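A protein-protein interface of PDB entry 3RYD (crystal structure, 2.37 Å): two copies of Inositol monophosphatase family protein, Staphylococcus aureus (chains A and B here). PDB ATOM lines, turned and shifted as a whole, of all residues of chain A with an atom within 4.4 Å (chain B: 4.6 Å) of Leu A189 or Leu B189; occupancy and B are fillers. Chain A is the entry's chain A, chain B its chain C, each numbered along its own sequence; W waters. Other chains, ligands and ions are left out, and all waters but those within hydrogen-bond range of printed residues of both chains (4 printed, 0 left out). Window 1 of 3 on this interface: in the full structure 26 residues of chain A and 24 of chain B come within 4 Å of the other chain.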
ATOM      1  N   SER A 166      -9.834 -21.370 -19.721  1.00  0.00           N
ATOM      2  CA  SER A 166      -9.958 -20.011 -19.226  1.00  0.00           C
ATOM      3  C   SER A 166     -10.195 -20.046 -17.728  1.00  0.00           C
ATOM      4  O   SER A 166     -10.890 -20.948 -17.207  1.00  0.00           O
ATOM      5  CB  SER A 166     -11.112 -19.303 -19.926  1.00  0.00           C
ATOM      6  OG  SER A 166     -11.915 -18.695 -18.970  1.00  0.00           O
ATOM      7  N   PHE A 167      -9.597 -19.061 -17.052  1.00  0.00           N
ATOM      8  CA  PHE A 167      -9.716 -18.860 -15.614  1.00  0.00           C
ATOM      9  C   PHE A 167      -8.933 -17.626 -15.279  1.00  0.00           C
ATOM     10  O   PHE A 167      -8.108 -17.141 -16.103  1.00  0.00           O
ATOM     11  CB  PHE A 167      -9.168 -20.055 -14.812  1.00  0.00           C
ATOM     12  CG  PHE A 167      -7.682 -20.369 -15.056  1.00  0.00           C
ATOM     13  CD1 PHE A 167      -6.677 -19.781 -14.265  1.00  0.00           C
ATOM     14  CD2 PHE A 167      -7.300 -21.291 -16.046  1.00  0.00           C
ATOM     15  CE1 PHE A 167      -5.293 -20.102 -14.474  1.00  0.00           C
ATOM     16  CE2 PHE A 167      -5.932 -21.594 -16.277  1.00  0.00           C
ATOM     17  CZ  PHE A 167      -4.932 -21.012 -15.503  1.00  0.00           C
ATOM     18  N   TYR A 187      -4.124 -21.096 -23.088  1.00  0.00           N
ATOM     19  CA  TYR A 187      -4.881 -20.330 -22.140  1.00  0.00           C
ATOM     20  C   TYR A 187      -5.349 -19.008 -22.748  1.00  0.00           C
ATOM     21  O   TYR A 187      -4.572 -18.280 -23.379  1.00  0.00           O
ATOM     22  CB  TYR A 187      -4.011 -20.057 -20.917  1.00  0.00           C
ATOM     23  CG  TYR A 187      -4.537 -18.986 -20.033  1.00  0.00           C
ATOM     24  CD1 TYR A 187      -5.438 -19.310 -19.035  1.00  0.00           C
ATOM     25  CD2 TYR A 187      -4.157 -17.631 -20.203  1.00  0.00           C
ATOM     26  CE1 TYR A 187      -5.940 -18.372 -18.204  1.00  0.00           C
ATOM     27  CE2 TYR A 187      -4.664 -16.660 -19.349  1.00  0.00           C
ATOM     28  CZ  TYR A 187      -5.572 -17.042 -18.341  1.00  0.00           C
ATOM     29  OH  TYR A 187      -6.138 -16.133 -17.443  1.00  0.00           O
ATOM     30  N   ARG A 188      -6.620 -18.710 -22.530  1.00  0.00           N
ATOM     31  CA  ARG A 188      -7.225 -17.463 -22.964  1.00  0.00           C
ATOM     32  C   ARG A 188      -8.161 -17.034 -21.842  1.00  0.00           C
ATOM     33  O   ARG A 188      -8.540 -17.865 -21.005  1.00  0.00           O
ATOM     34  CB  ARG A 188      -7.986 -17.687 -24.283  1.00  0.00           C
ATOM     35  CG  ARG A 188      -7.113 -18.177 -25.474  1.00  0.00           C
ATOM     36  CD  ARG A 188      -5.698 -17.470 -25.575  1.00  0.00           C
ATOM     37  NE  ARG A 188      -4.701 -18.231 -26.376  1.00  0.00           N
ATOM     38  CZ  ARG A 188      -4.928 -18.392 -27.654  1.00  0.00           C
ATOM     39  NH1 ARG A 188      -6.042 -17.831 -28.123  1.00  0.00           N
ATOM     40  NH2 ARG A 188      -4.129 -19.082 -28.443  1.00  0.00           N
ATOM     41  N   LEU A 189      -8.503 -15.741 -21.800  1.00  0.00           N
ATOM     42  CA  LEU A 189      -9.571 -15.218 -20.929  1.00  0.00           C
ATOM     43  C   LEU A 189     -10.423 -14.132 -21.593  1.00  0.00           C
ATOM     44  O   LEU A 189      -9.892 -13.113 -22.036  1.00  0.00           O
ATOM     45  CB  LEU A 189      -8.998 -14.671 -19.611  1.00  0.00           C
ATOM     46  CG  LEU A 189      -9.973 -14.148 -18.524  1.00  0.00           C
ATOM     47  CD1 LEU A 189     -11.035 -15.149 -18.015  1.00  0.00           C
ATOM     48  CD2 LEU A 189      -9.182 -13.589 -17.325  1.00  0.00           C
ATOM     49  N   VAL A 190     -11.748 -14.329 -21.633  1.00  0.00           N
ATOM     50  CA  VAL A 190     -12.636 -13.285 -22.175  1.00  0.00           C
ATOM     51  C   VAL A 190     -12.927 -12.252 -21.067  1.00  0.00           C
ATOM     52  O   VAL A 190     -12.797 -11.028 -21.256  1.00  0.00           O
ATOM     53  CB  VAL A 190     -13.948 -13.874 -22.795  1.00  0.00           C
ATOM     54  CG1 VAL A 190     -14.841 -12.775 -23.261  1.00  0.00           C
ATOM     55  CG2 VAL A 190     -13.618 -14.839 -23.926  1.00  0.00           C
ATOM     56  N   GLY A 191     -13.292 -12.769 -19.906  1.00  0.00           N
ATOM     57  CA  GLY A 191     -13.457 -11.931 -18.733  1.00  0.00           C
ATOM     58  C   GLY A 191     -14.888 -11.658 -18.297  1.00  0.00           C
ATOM     59  O   GLY A 191     -15.113 -10.888 -17.353  1.00  0.00           O
ATOM     60  N   ASP A 196     -17.030 -16.673 -21.223  1.00  0.00           N
ATOM     61  CA  ASP A 196     -16.062 -17.759 -21.063  1.00  0.00           C
ATOM     62  C   ASP A 196     -16.815 -19.135 -20.929  1.00  0.00           C
ATOM     63  O   ASP A 196     -16.316 -20.166 -21.398  1.00  0.00           O
ATOM     64  CB  ASP A 196     -15.161 -17.511 -19.832  1.00  0.00           C
ATOM     65  CG  ASP A 196     -14.152 -16.352 -20.027  1.00  0.00           C
ATOM     66  OD1 ASP A 196     -13.074 -16.577 -20.655  1.00  0.00           O
ATOM     67  OD2 ASP A 196     -14.416 -15.216 -19.536  1.00  0.00           O
ATOM     68  N   SER B 166      -2.582  -7.228 -21.740  1.00  0.00           N
ATOM     69  CA  SER B 166      -2.568  -8.497 -22.438  1.00  0.00           C
ATOM     70  C   SER B 166      -1.117  -8.883 -22.748  1.00  0.00           C
ATOM     71  O   SER B 166      -0.333  -8.041 -23.212  1.00  0.00           O
ATOM     72  CB  SER B 166      -3.401  -8.388 -23.713  1.00  0.00           C
ATOM     73  OG  SER B 166      -2.759  -9.081 -24.758  1.00  0.00           O
ATOM     74  N   PHE B 167      -0.776 -10.131 -22.406  1.00  0.00           N
ATOM     75  CA  PHE B 167       0.475 -10.772 -22.743  1.00  0.00           C
ATOM     76  C   PHE B 167       0.341 -12.283 -22.597  1.00  0.00           C
ATOM     77  O   PHE B 167      -0.606 -12.785 -21.960  1.00  0.00           O
ATOM     78  CB  PHE B 167       1.598 -10.281 -21.839  1.00  0.00           C
ATOM     79  CG  PHE B 167       1.306 -10.386 -20.333  1.00  0.00           C
ATOM     80  CD1 PHE B 167       1.742 -11.487 -19.611  1.00  0.00           C
ATOM     81  CD2 PHE B 167       0.643  -9.357 -19.656  1.00  0.00           C
ATOM     82  CE1 PHE B 167       1.499 -11.613 -18.237  1.00  0.00           C
ATOM     83  CE2 PHE B 167       0.399  -9.447 -18.270  1.00  0.00           C
ATOM     84  CZ  PHE B 167       0.837 -10.588 -17.543  1.00  0.00           C
ATOM     85  N   TYR B 187      -6.107  -8.265 -16.326  1.00  0.00           N
ATOM     86  CA  TYR B 187      -5.413  -8.992 -17.355  1.00  0.00           C
ATOM     87  C   TYR B 187      -6.452  -9.655 -18.250  1.00  0.00           C
ATOM     88  O   TYR B 187      -7.450 -10.180 -17.760  1.00  0.00           O
ATOM     89  CB  TYR B 187      -4.516 -10.049 -16.698  1.00  0.00           C
ATOM     90  CG  TYR B 187      -3.933 -11.077 -17.648  1.00  0.00           C
ATOM     91  CD1 TYR B 187      -2.858 -10.777 -18.490  1.00  0.00           C
ATOM     92  CD2 TYR B 187      -4.437 -12.350 -17.679  1.00  0.00           C
ATOM     93  CE1 TYR B 187      -2.321 -11.744 -19.362  1.00  0.00           C
ATOM     94  CE2 TYR B 187      -3.928 -13.308 -18.534  1.00  0.00           C
ATOM     95  CZ  TYR B 187      -2.873 -13.007 -19.375  1.00  0.00           C
ATOM     96  OH  TYR B 187      -2.400 -14.021 -20.177  1.00  0.00           O
ATOM     97  N   ARG B 188      -6.226  -9.616 -19.561  1.00  0.00           N
ATOM     98  CA  ARG B 188      -7.064 -10.358 -20.515  1.00  0.00           C
ATOM     99  C   ARG B 188      -6.145 -10.898 -21.582  1.00  0.00           C
ATOM    100  O   ARG B 188      -4.962 -10.504 -21.659  1.00  0.00           O
ATOM    101  CB  ARG B 188      -8.112  -9.449 -21.191  1.00  0.00           C
ATOM    102  CG  ARG B 188      -9.096  -8.676 -20.302  1.00  0.00           C
ATOM    103  CD  ARG B 188     -10.333  -9.457 -19.919  1.00  0.00           C
ATOM    104  NE  ARG B 188     -10.135  -9.716 -18.518  1.00  0.00           N
ATOM    105  CZ  ARG B 188     -10.777  -9.145 -17.520  1.00  0.00           C
ATOM    106  NH1 ARG B 188     -11.770  -8.314 -17.731  1.00  0.00           N
ATOM    107  NH2 ARG B 188     -10.397  -9.443 -16.298  1.00  0.00           N
ATOM    108  N   LEU B 189      -6.667 -11.797 -22.414  1.00  0.00           N
ATOM    109  CA  LEU B 189      -5.920 -12.273 -23.594  1.00  0.00           C
ATOM    110  C   LEU B 189      -6.850 -12.769 -24.684  1.00  0.00           C
ATOM    111  O   LEU B 189      -7.645 -13.662 -24.445  1.00  0.00           O
ATOM    112  CB  LEU B 189      -4.923 -13.390 -23.222  1.00  0.00           C
ATOM    113  CG  LEU B 189      -4.046 -13.894 -24.402  1.00  0.00           C
ATOM    114  CD1 LEU B 189      -3.137 -12.764 -24.943  1.00  0.00           C
ATOM    115  CD2 LEU B 189      -3.218 -15.118 -24.014  1.00  0.00           C
ATOM    116  N   VAL B 190      -6.741 -12.210 -25.880  1.00  0.00           N
ATOM    117  CA  VAL B 190      -7.509 -12.693 -27.049  1.00  0.00           C
ATOM    118  C   VAL B 190      -6.754 -13.827 -27.769  1.00  0.00           C
ATOM    119  O   VAL B 190      -7.359 -14.823 -28.118  1.00  0.00           O
ATOM    120  CB  VAL B 190      -7.792 -11.522 -28.051  1.00  0.00           C
ATOM    121  CG1 VAL B 190      -8.608 -11.991 -29.293  1.00  0.00           C
ATOM    122  CG2 VAL B 190      -8.548 -10.423 -27.357  1.00  0.00           C
ATOM    123  N   GLY B 191      -5.441 -13.669 -28.000  1.00  0.00           N
ATOM    124  CA  GLY B 191      -4.604 -14.742 -28.502  1.00  0.00           C
ATOM    125  C   GLY B 191      -4.200 -14.606 -29.954  1.00  0.00           C
ATOM    126  O   GLY B 191      -3.690 -15.550 -30.566  1.00  0.00           O
ATOM    127  N   ASP B 196      -5.158  -8.378 -30.208  1.00  0.00           N
ATOM    128  CA  ASP B 196      -4.755  -7.804 -28.938  1.00  0.00           C
ATOM    129  C   ASP B 196      -4.187  -6.425 -29.162  1.00  0.00           C
ATOM    130  O   ASP B 196      -4.286  -5.585 -28.286  1.00  0.00           O
ATOM    131  CB  ASP B 196      -3.654  -8.626 -28.302  1.00  0.00           C
ATOM    132  CG  ASP B 196      -4.157  -9.813 -27.576  1.00  0.00           C
ATOM    133  OD1 ASP B 196      -4.845  -9.620 -26.533  1.00  0.00           O
ATOM    134  OD2 ASP B 196      -3.824 -10.929 -28.031  1.00  0.00           O
HETATM  135  O   HOH W   1     -15.091  -8.140 -17.016  1.00  0.00           O
HETATM  136  O   HOH W   2      -4.322 -18.226 -31.482  1.00  0.00           O
HETATM  137  O   HOH W   3     -10.065 -14.767 -25.016  1.00  0.00           O
HETATM  138  O   HOH W   4      -9.851 -11.030 -24.149  1.00  0.00           O
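The backbone carbonyl oxygen (O) of Val B190 lies within hydrogen-bond range of the guanidinium group (NH1) of Arg A188.
N of Leu A189 is in hydrogen-bond range of O of Leu B189 (3.5 Å).
O of Phe A167 sits at hydrogen-bond distance from OH of Tyr A187 (2.6 Å).
N of Gly A191 sits at hydrogen-bond distance from OD2 of Asp A196 (2.7 Å).
N of Gly B191 sits at hydrogen-bond distance from OD2 of Asp B196 (3.2 Å).
The side-chain carboxylate (OD1) of Asp A196 lies within hydrogen-bond range of the backbone NH (N) of Val A190.
The side-chain hydroxyl of Tyr B187 sits at hydrogen-bond distance from the backbone carbonyl oxygen of Phe B167, at 2.8 Å.
OD1 of Asp B196 sits at hydrogen-bond distance from N of Val B190 (3.3 Å).
CE2 of Tyr A187 touches CE2 of Tyr B187 (3.5 Å).
Tyr A187 touches Leu B189 (O to CD2, 3.5 Å).
Leu B189 touches Arg A188 (CD2 to CD, 3.8 Å).
Arg A188 touches Gly B191.
Leu A189 touches Tyr B187 (CD2 to O, 3.8 Å).
Val A190 touches Arg B188 (O to CD, 3.2 Å).
NE of Arg B188 touches CA of Gly A191, at 3.999 Å.
Tyr A187 touches its own counterpart, Tyr B187.
Tyr A187 touches Leu B189, and with the chains exchanged Leu A189 touches Tyr B187.
Arg A188 touches Leu B189, but with the chains exchanged Leu A189 does not touch Arg B188 (4.2 Å).
Leu A189 touches its own counterpart, Leu B189.
Positions printed for both chains: 166, 167, 187, 188, 189, 190, 191 and 196.
Of the 9 pairs that touch across the chains among the printed residues, 8 have their exchanged pair printed and touching as well.
Hydrophobic or aromatic side chains of chain B that line the printed part of chain A: Tyr B187 and Leu B189.
Among the printed residues, 9 pairs touch across the chains.
Among the printed residues, no Asp or Glu carboxylate lies within 4 Å of a Lys or Arg side-chain nitrogen of the other chain.
Water W3 lies within hydrogen-bond range of O of Leu B189 (2.7 Å) and O of Leu A189 (3.4 Å).
Water W1 bridges the backbone carbonyl oxygen of Gly A191 and the guanidinium group of Arg B188.
Water W2 bridges the backbone carbonyl oxygen of Gly B191 (2.9 Å) and the guanidinium group of Arg A188 (3.2 Å).
Water W4 bridges O of Leu A189 (3.0 Å) and O of Leu B189 (3.4 Å).
Ser A166 touches none of the printed residues of chain B.
Printed residues of chain B within 4 Å of Arg A188: Leu B189 (3.8 Å), Val B190 (3.3 Å) and Gly B191 (3.4 Å).
Of chain B, only Tyr B187 and Leu B189 come within 4 Å of Leu A189.
Of the printed residues of chain B, Val A190 touches Arg B188.
Asp A196 touches none of the printed residues of chain B.
Of the printed residues of chain A, Tyr B187 touches Tyr A187 and Leu A189.
Leu B189 touches three residues of chain A.
The nearest printed residue of chain A that does not touch Leu B189 is Val A190 (5.0 Å).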
